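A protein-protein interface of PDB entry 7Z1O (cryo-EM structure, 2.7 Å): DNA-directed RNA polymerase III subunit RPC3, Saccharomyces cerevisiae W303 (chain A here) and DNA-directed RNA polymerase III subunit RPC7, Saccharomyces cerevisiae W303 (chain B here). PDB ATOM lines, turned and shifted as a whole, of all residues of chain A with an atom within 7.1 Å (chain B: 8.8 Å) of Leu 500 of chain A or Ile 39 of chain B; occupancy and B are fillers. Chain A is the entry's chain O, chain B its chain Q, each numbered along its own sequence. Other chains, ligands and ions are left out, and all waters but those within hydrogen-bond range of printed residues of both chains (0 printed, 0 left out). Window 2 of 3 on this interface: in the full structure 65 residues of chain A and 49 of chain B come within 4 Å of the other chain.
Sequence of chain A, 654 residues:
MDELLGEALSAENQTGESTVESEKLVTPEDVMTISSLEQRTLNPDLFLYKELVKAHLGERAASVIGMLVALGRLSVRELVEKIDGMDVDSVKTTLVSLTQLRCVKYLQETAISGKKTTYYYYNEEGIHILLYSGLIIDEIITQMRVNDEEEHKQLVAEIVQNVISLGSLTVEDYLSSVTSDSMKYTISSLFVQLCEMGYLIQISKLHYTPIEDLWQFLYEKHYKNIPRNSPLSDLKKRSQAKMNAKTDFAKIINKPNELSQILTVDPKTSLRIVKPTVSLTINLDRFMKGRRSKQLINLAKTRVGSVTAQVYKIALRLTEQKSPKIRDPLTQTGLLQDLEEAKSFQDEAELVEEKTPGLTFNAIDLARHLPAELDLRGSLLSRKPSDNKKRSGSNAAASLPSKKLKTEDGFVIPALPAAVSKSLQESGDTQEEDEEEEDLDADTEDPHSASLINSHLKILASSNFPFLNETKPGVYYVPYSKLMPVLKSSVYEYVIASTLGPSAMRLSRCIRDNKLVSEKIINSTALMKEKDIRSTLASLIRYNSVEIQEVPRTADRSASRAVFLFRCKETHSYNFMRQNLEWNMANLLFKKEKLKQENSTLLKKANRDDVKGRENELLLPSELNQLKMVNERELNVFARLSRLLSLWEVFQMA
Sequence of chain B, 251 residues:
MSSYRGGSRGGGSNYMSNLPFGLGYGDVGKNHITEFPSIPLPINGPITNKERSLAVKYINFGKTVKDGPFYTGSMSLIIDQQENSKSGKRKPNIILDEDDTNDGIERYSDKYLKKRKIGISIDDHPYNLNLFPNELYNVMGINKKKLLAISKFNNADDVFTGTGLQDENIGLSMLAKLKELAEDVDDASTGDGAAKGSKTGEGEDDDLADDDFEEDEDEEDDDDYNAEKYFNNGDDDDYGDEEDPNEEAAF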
ATOM      1  N   VAL A 495      14.570 -17.734 -25.469  1.00  0.00           N
ATOM      2  CA  VAL A 495      13.945 -16.622 -26.181  1.00  0.00           C
ATOM      3  C   VAL A 495      12.556 -16.354 -25.617  1.00  0.00           C
ATOM      4  O   VAL A 495      12.178 -15.198 -25.376  1.00  0.00           O
ATOM      5  CB  VAL A 495      13.896 -16.900 -27.695  1.00  0.00           C
ATOM      6  CG1 VAL A 495      12.898 -15.984 -28.367  1.00  0.00           C
ATOM      7  CG2 VAL A 495      15.263 -16.719 -28.314  1.00  0.00           C
ATOM      8  N   ILE A 496      11.780 -17.418 -25.379  1.00  0.00           N
ATOM      9  CA  ILE A 496      10.460 -17.241 -24.773  1.00  0.00           C
ATOM     10  C   ILE A 496      10.581 -16.660 -23.369  1.00  0.00           C
ATOM     11  O   ILE A 496       9.765 -15.830 -22.955  1.00  0.00           O
ATOM     12  CB  ILE A 496       9.681 -18.567 -24.772  1.00  0.00           C
ATOM     13  CG1 ILE A 496       9.375 -19.005 -26.193  1.00  0.00           C
ATOM     14  CG2 ILE A 496       8.377 -18.439 -24.032  1.00  0.00           C
ATOM     15  CD1 ILE A 496       8.761 -20.348 -26.228  1.00  0.00           C
ATOM     16  N   ALA A 497      11.598 -17.080 -22.617  1.00  0.00           N
ATOM     17  CA  ALA A 497      11.812 -16.525 -21.284  1.00  0.00           C
ATOM     18  C   ALA A 497      12.119 -15.037 -21.343  1.00  0.00           C
ATOM     19  O   ALA A 497      11.615 -14.256 -20.528  1.00  0.00           O
ATOM     20  CB  ALA A 497      12.950 -17.261 -20.592  1.00  0.00           C
ATOM     21  N   SER A 498      12.949 -14.628 -22.298  1.00  0.00           N
ATOM     22  CA  SER A 498      13.306 -13.224 -22.425  1.00  0.00           C
ATOM     23  C   SER A 498      12.143 -12.375 -22.917  1.00  0.00           C
ATOM     24  O   SER A 498      12.050 -11.196 -22.560  1.00  0.00           O
ATOM     25  CB  SER A 498      14.497 -13.076 -23.366  1.00  0.00           C
ATOM     26  OG  SER A 498      14.130 -13.371 -24.702  1.00  0.00           O
ATOM     27  N   THR A 499      11.254 -12.942 -23.733  1.00  0.00           N
ATOM     28  CA  THR A 499      10.162 -12.156 -24.298  1.00  0.00           C
ATOM     29  C   THR A 499       8.902 -12.198 -23.434  1.00  0.00           C
ATOM     30  O   THR A 499       8.451 -11.163 -22.934  1.00  0.00           O
ATOM     31  CB  THR A 499       9.850 -12.640 -25.718  1.00  0.00           C
ATOM     32  OG1 THR A 499       9.560 -14.043 -25.696  1.00  0.00           O
ATOM     33  CG2 THR A 499      11.036 -12.387 -26.632  1.00  0.00           C
ATOM     34  N   LEU A 500       8.331 -13.385 -23.242  1.00  0.00           N
ATOM     35  CA  LEU A 500       7.059 -13.537 -22.548  1.00  0.00           C
ATOM     36  C   LEU A 500       7.200 -13.761 -21.048  1.00  0.00           C
ATOM     37  O   LEU A 500       6.186 -13.754 -20.342  1.00  0.00           O
ATOM     38  CB  LEU A 500       6.268 -14.700 -23.155  1.00  0.00           C
ATOM     39  CG  LEU A 500       5.957 -14.606 -24.647  1.00  0.00           C
ATOM     40  CD1 LEU A 500       5.387 -15.915 -25.155  1.00  0.00           C
ATOM     41  CD2 LEU A 500       4.998 -13.464 -24.918  1.00  0.00           C
ATOM     42  N   GLY A 501       8.414 -13.962 -20.540  1.00  0.00           N
ATOM     43  CA  GLY A 501       8.622 -14.113 -19.119  1.00  0.00           C
ATOM     44  C   GLY A 501       9.086 -15.498 -18.714  1.00  0.00           C
ATOM     45  O   GLY A 501       8.928 -16.474 -19.453  1.00  0.00           O
ATOM     46  N   PRO A 502       9.695 -15.601 -17.528  1.00  0.00           N
ATOM     47  CA  PRO A 502      10.118 -16.920 -17.027  1.00  0.00           C
ATOM     48  C   PRO A 502       8.966 -17.878 -16.773  1.00  0.00           C
ATOM     49  O   PRO A 502       9.149 -19.100 -16.888  1.00  0.00           O
ATOM     50  CB  PRO A 502      10.865 -16.577 -15.731  1.00  0.00           C
ATOM     51  CG  PRO A 502      10.333 -15.245 -15.324  1.00  0.00           C
ATOM     52  CD  PRO A 502      10.033 -14.514 -16.594  1.00  0.00           C
ATOM     53  N   SER A 503       7.787 -17.362 -16.416  1.00  0.00           N
ATOM     54  CA  SER A 503       6.621 -18.223 -16.252  1.00  0.00           C
ATOM     55  C   SER A 503       6.248 -18.903 -17.559  1.00  0.00           C
ATOM     56  O   SER A 503       5.752 -20.035 -17.554  1.00  0.00           O
ATOM     57  CB  SER A 503       5.441 -17.415 -15.718  1.00  0.00           C
ATOM     58  OG  SER A 503       4.279 -18.218 -15.621  1.00  0.00           O
ATOM     59  N   ALA A 504       6.489 -18.233 -18.688  1.00  0.00           N
ATOM     60  CA  ALA A 504       6.281 -18.865 -19.985  1.00  0.00           C
ATOM     61  C   ALA A 504       7.254 -20.018 -20.203  1.00  0.00           C
ATOM     62  O   ALA A 504       6.868 -21.063 -20.744  1.00  0.00           O
ATOM     63  CB  ALA A 504       6.401 -17.826 -21.095  1.00  0.00           C
ATOM     64  N   MET A 505       8.515 -19.857 -19.777  1.00  0.00           N
ATOM     65  CA  MET A 505       9.455 -20.977 -19.813  1.00  0.00           C
ATOM     66  C   MET A 505       8.947 -22.137 -18.974  1.00  0.00           C
ATOM     67  O   MET A 505       9.004 -23.299 -19.396  1.00  0.00           O
ATOM     68  CB  MET A 505      10.835 -20.575 -19.286  1.00  0.00           C
ATOM     69  CG  MET A 505      11.902 -21.592 -19.684  1.00  0.00           C
ATOM     70  SD  MET A 505      13.461 -21.633 -18.767  1.00  0.00           S
ATOM     71  CE  MET A 505      13.801 -19.918 -18.443  1.00  0.00           C
ATOM     72  N   THR A 536      -0.941 -17.116 -19.430  1.00  0.00           N
ATOM     73  CA  THR A 536       0.339 -17.478 -20.026  1.00  0.00           C
ATOM     74  C   THR A 536       0.162 -18.437 -21.195  1.00  0.00           C
ATOM     75  O   THR A 536       0.825 -18.288 -22.227  1.00  0.00           O
ATOM     76  CB  THR A 536       1.257 -18.087 -18.967  1.00  0.00           C
ATOM     77  OG1 THR A 536       1.277 -17.245 -17.809  1.00  0.00           O
ATOM     78  CG2 THR A 536       2.668 -18.219 -19.505  1.00  0.00           C
ATOM     79  N   SER A 539      -1.204 -16.567 -24.149  1.00  0.00           N
ATOM     80  CA  SER A 539      -0.125 -15.858 -24.829  1.00  0.00           C
ATOM     81  C   SER A 539       0.746 -16.815 -25.639  1.00  0.00           C
ATOM     82  O   SER A 539       1.181 -16.482 -26.746  1.00  0.00           O
ATOM     83  CB  SER A 539       0.720 -15.091 -23.815  1.00  0.00           C
ATOM     84  OG  SER A 539       1.799 -14.428 -24.449  1.00  0.00           O
ATOM     85  N   LEU A 540       1.010 -18.009 -25.102  1.00  0.00           N
ATOM     86  CA  LEU A 540       1.883 -18.960 -25.787  1.00  0.00           C
ATOM     87  C   LEU A 540       1.224 -19.561 -27.023  1.00  0.00           C
ATOM     88  O   LEU A 540       1.925 -19.961 -27.960  1.00  0.00           O
ATOM     89  CB  LEU A 540       2.299 -20.077 -24.830  1.00  0.00           C
ATOM     90  CG  LEU A 540       3.439 -19.798 -23.852  1.00  0.00           C
ATOM     91  CD1 LEU A 540       3.568 -20.940 -22.866  1.00  0.00           C
ATOM     92  CD2 LEU A 540       4.744 -19.576 -24.586  1.00  0.00           C
ATOM     93  N   ILE A 541      -0.108 -19.649 -27.038  1.00  0.00           N
ATOM     94  CA  ILE A 541      -0.819 -20.223 -28.178  1.00  0.00           C
ATOM     95  C   ILE A 541      -0.627 -19.364 -29.423  1.00  0.00           C
ATOM     96  O   ILE A 541      -0.510 -19.888 -30.539  1.00  0.00           O
ATOM     97  CB  ILE A 541      -2.311 -20.416 -27.817  1.00  0.00           C
ATOM     98  CG1 ILE A 541      -2.495 -21.679 -26.977  1.00  0.00           C
ATOM     99  CG2 ILE A 541      -3.184 -20.531 -29.046  1.00  0.00           C
ATOM    100  CD1 ILE A 541      -3.736 -21.658 -26.118  1.00  0.00           C
ATOM    101  N   TYR A 543       1.917 -17.974 -30.538  1.00  0.00           N
ATOM    102  CA  TYR A 543       3.226 -18.154 -31.152  1.00  0.00           C
ATOM    103  C   TYR A 543       3.532 -19.615 -31.470  1.00  0.00           C
ATOM    104  O   TYR A 543       4.707 -19.994 -31.535  1.00  0.00           O
ATOM    105  CB  TYR A 543       4.315 -17.576 -30.248  1.00  0.00           C
ATOM    106  CG  TYR A 543       4.114 -16.120 -29.904  1.00  0.00           C
ATOM    107  CD1 TYR A 543       4.435 -15.120 -30.811  1.00  0.00           C
ATOM    108  CD2 TYR A 543       3.597 -15.746 -28.673  1.00  0.00           C
ATOM    109  CE1 TYR A 543       4.249 -13.789 -30.498  1.00  0.00           C
ATOM    110  CE2 TYR A 543       3.407 -14.419 -28.352  1.00  0.00           C
ATOM    111  CZ  TYR A 543       3.734 -13.445 -29.266  1.00  0.00           C
ATOM    112  OH  TYR A 543       3.544 -12.121 -28.946  1.00  0.00           O
ATOM    113  N   SER A 545       3.490 -22.090 -29.657  1.00  0.00           N
ATOM    114  CA  SER A 545       4.196 -22.797 -28.597  1.00  0.00           C
ATOM    115  C   SER A 545       3.358 -23.931 -28.026  1.00  0.00           C
ATOM    116  O   SER A 545       3.880 -25.020 -27.761  1.00  0.00           O
ATOM    117  CB  SER A 545       4.593 -21.822 -27.490  1.00  0.00           C
ATOM    118  OG  SER A 545       5.323 -20.730 -28.017  1.00  0.00           O
ATOM    119  N   PHE B  36       0.599  -1.663 -32.365  1.00  0.00           N
ATOM    120  CA  PHE B  36       2.002  -1.508 -32.040  1.00  0.00           C
ATOM    121  C   PHE B  36       2.440  -2.563 -31.031  1.00  0.00           C
ATOM    122  O   PHE B  36       1.799  -2.727 -29.988  1.00  0.00           O
ATOM    123  CB  PHE B  36       2.277  -0.109 -31.473  1.00  0.00           C
ATOM    124  CG  PHE B  36       1.874   1.006 -32.394  1.00  0.00           C
ATOM    125  CD1 PHE B  36       2.757   1.493 -33.342  1.00  0.00           C
ATOM    126  CD2 PHE B  36       0.612   1.569 -32.311  1.00  0.00           C
ATOM    127  CE1 PHE B  36       2.390   2.516 -34.191  1.00  0.00           C
ATOM    128  CE2 PHE B  36       0.239   2.593 -33.158  1.00  0.00           C
ATOM    129  CZ  PHE B  36       1.129   3.068 -34.098  1.00  0.00           C
ATOM    130  N   PRO B  37       3.518  -3.288 -31.312  1.00  0.00           N
ATOM    131  CA  PRO B  37       3.970  -4.336 -30.393  1.00  0.00           C
ATOM    132  C   PRO B  37       4.589  -3.760 -29.130  1.00  0.00           C
ATOM    133  O   PRO B  37       5.002  -2.601 -29.073  1.00  0.00           O
ATOM    134  CB  PRO B  37       5.006  -5.102 -31.218  1.00  0.00           C
ATOM    135  CG  PRO B  37       5.509  -4.096 -32.195  1.00  0.00           C
ATOM    136  CD  PRO B  37       4.339  -3.228 -32.532  1.00  0.00           C
ATOM    137  N   SER B  38       4.650  -4.607 -28.094  1.00  0.00           N
ATOM    138  CA  SER B  38       5.189  -4.182 -26.808  1.00  0.00           C
ATOM    139  C   SER B  38       6.096  -5.230 -26.169  1.00  0.00           C
ATOM    140  O   SER B  38       6.375  -5.140 -24.968  1.00  0.00           O
ATOM    141  CB  SER B  38       4.056  -3.833 -25.839  1.00  0.00           C
ATOM    142  OG  SER B  38       3.272  -2.760 -26.334  1.00  0.00           O
ATOM    143  N   ILE B  39       6.566  -6.215 -26.929  1.00  0.00           N
ATOM    144  CA  ILE B  39       7.429  -7.266 -26.391  1.00  0.00           C
ATOM    145  C   ILE B  39       8.765  -7.236 -27.124  1.00  0.00           C
ATOM    146  O   ILE B  39       8.887  -7.827 -28.207  1.00  0.00           O
ATOM    147  CB  ILE B  39       6.768  -8.647 -26.506  1.00  0.00           C
ATOM    148  CG1 ILE B  39       5.345  -8.611 -25.951  1.00  0.00           C
ATOM    149  CG2 ILE B  39       7.587  -9.687 -25.773  1.00  0.00           C
ATOM    150  CD1 ILE B  39       4.625  -9.933 -26.037  1.00  0.00           C
ATOM    151  N   PRO B  40       9.782  -6.570 -26.588  1.00  0.00           N
ATOM    152  CA  PRO B  40      11.053  -6.463 -27.305  1.00  0.00           C
ATOM    153  C   PRO B  40      12.012  -7.598 -26.983  1.00  0.00           C
ATOM    154  O   PRO B  40      12.048  -8.128 -25.870  1.00  0.00           O
ATOM    155  CB  PRO B  40      11.611  -5.123 -26.814  1.00  0.00           C
ATOM    156  CG  PRO B  40      11.089  -5.010 -25.424  1.00  0.00           C
ATOM    157  CD  PRO B  40       9.754  -5.719 -25.387  1.00  0.00           C
ATOM    158  N   LEU B  41      12.795  -7.969 -27.991  1.00  0.00           N
ATOM    159  CA  LEU B  41      13.894  -8.902 -27.821  1.00  0.00           C
ATOM    160  C   LEU B  41      15.046  -8.219 -27.087  1.00  0.00           C
ATOM    161  O   LEU B  41      15.174  -6.992 -27.125  1.00  0.00           O
ATOM    162  CB  LEU B  41      14.354  -9.412 -29.185  1.00  0.00           C
ATOM    163  CG  LEU B  41      13.615 -10.617 -29.773  1.00  0.00           C
ATOM    164  CD1 LEU B  41      13.963 -10.796 -31.239  1.00  0.00           C
ATOM    165  CD2 LEU B  41      13.925 -11.880 -28.994  1.00  0.00           C
ATOM    166  N   PRO B  42      15.903  -8.985 -26.405  1.00  0.00           N
ATOM    167  CA  PRO B  42      17.043  -8.376 -25.706  1.00  0.00           C
ATOM    168  C   PRO B  42      18.168  -7.920 -26.619  1.00  0.00           C
ATOM    169  O   PRO B  42      19.197  -7.451 -26.117  1.00  0.00           O
ATOM    170  CB  PRO B  42      17.532  -9.502 -24.779  1.00  0.00           C
ATOM    171  CG  PRO B  42      16.515 -10.565 -24.851  1.00  0.00           C
ATOM    172  CD  PRO B  42      15.824 -10.430 -26.150  1.00  0.00           C
ATOM    173  N   ASN B  44      18.371  -5.367 -28.409  1.00  0.00           N
ATOM    174  CA  ASN B  44      18.344  -3.925 -28.623  1.00  0.00           C
ATOM    175  C   ASN B  44      19.249  -3.165 -27.663  1.00  0.00           C
ATOM    176  O   ASN B  44      19.003  -1.983 -27.391  1.00  0.00           O
ATOM    177  CB  ASN B  44      16.909  -3.413 -28.517  1.00  0.00           C
ATOM    178  CG  ASN B  44      15.912  -4.352 -29.151  1.00  0.00           C
ATOM    179  OD1 ASN B  44      16.044  -4.719 -30.317  1.00  0.00           O
ATOM    180  ND2 ASN B  44      14.903  -4.748 -28.387  1.00  0.00           N
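Of the printed residues of chain B, Ser 498 of chain A touches Pro 42 (3.5 Å).
Of chain B, only Ile 39 and Leu 41 come within 4 Å of Thr 499 of chain A.
Leu 500 of chain A touches just one residue of chain B: Ile 39.
No residue of chain B comes within 4 Å of Gly 501 of chain A.
Of the printed residues of chain B, Tyr 543 of chain A touches Ile 39.
Ser 545 of chain A touches none of the printed residues of chain B.
Of chain A, only Thr 499 (3.3 Å), Leu 500 (3.7 Å) and Tyr 543 (3.8 Å) come within 4 Å of Ile 39 of chain B.
Of the printed residues of chain A, Leu 41 of chain B touches Thr 499 (3.8 Å).
Of the printed residues of chain A, Pro 42 of chain B touches Ser 498.
The nearest residue of chain B that does not touch Leu 500 of chain A is Pro 40 of chain B (7.0 Å).
The nearest residue of chain A that does not touch Ile 39 of chain B is Ser 539 of chain A (5.5 Å).
The nearest printed residue of chain A that does not touch Pro 42 of chain B is Thr 499 of chain A (5.2 Å).
CB of Ser 498 of chain A touches CG of Pro 42 of chain B, 3.5 Å away.
O of Thr 499 of chain A touches CG2 of Ile 39 of chain B, at 3.3 Å.
CG2 of Thr 499 of chain A touches CD2 of Leu 41 of chain B (3.8 Å).
Leu 500 of chain A touches Ile 39 of chain B (CD2 to CD1, 3.7 Å).
Ile 39 of chain B touches Tyr 543 of chain A.
OG of Ser 498 of chain A is in hydrogen-bond range of O of Val 495 of chain A (2.8 Å).
The backbone carbonyl oxygen (O) of Val 495 of chain A is in hydrogen-bond range of the side-chain hydroxyl (OG1) of Thr 499 of chain A (2.9 Å).
The backbone carbonyl oxygen of Ile 496 of chain A sits at hydrogen-bond distance from the side-chain hydroxyl of Thr 499 of chain A, 3.3 Å away.
O of Leu 41 of chain B sits at hydrogen-bond distance from ND2 of Asn 44 of chain B (2.6 Å).
Hydrophobic or aromatic side chains of chain B within 4 Å of the printed part of chain A: Ile 39, Leu 41 and Pro 42.
Along chain B the printed residues that touch a printed residue of chain A span positions 39 to 42.
Among the printed residues, 5 pairs touch across the chains.
Among the printed residues, no Asp or Glu carboxylate lies within 4 Å of a Lys or Arg side-chain nitrogen of the other chain.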
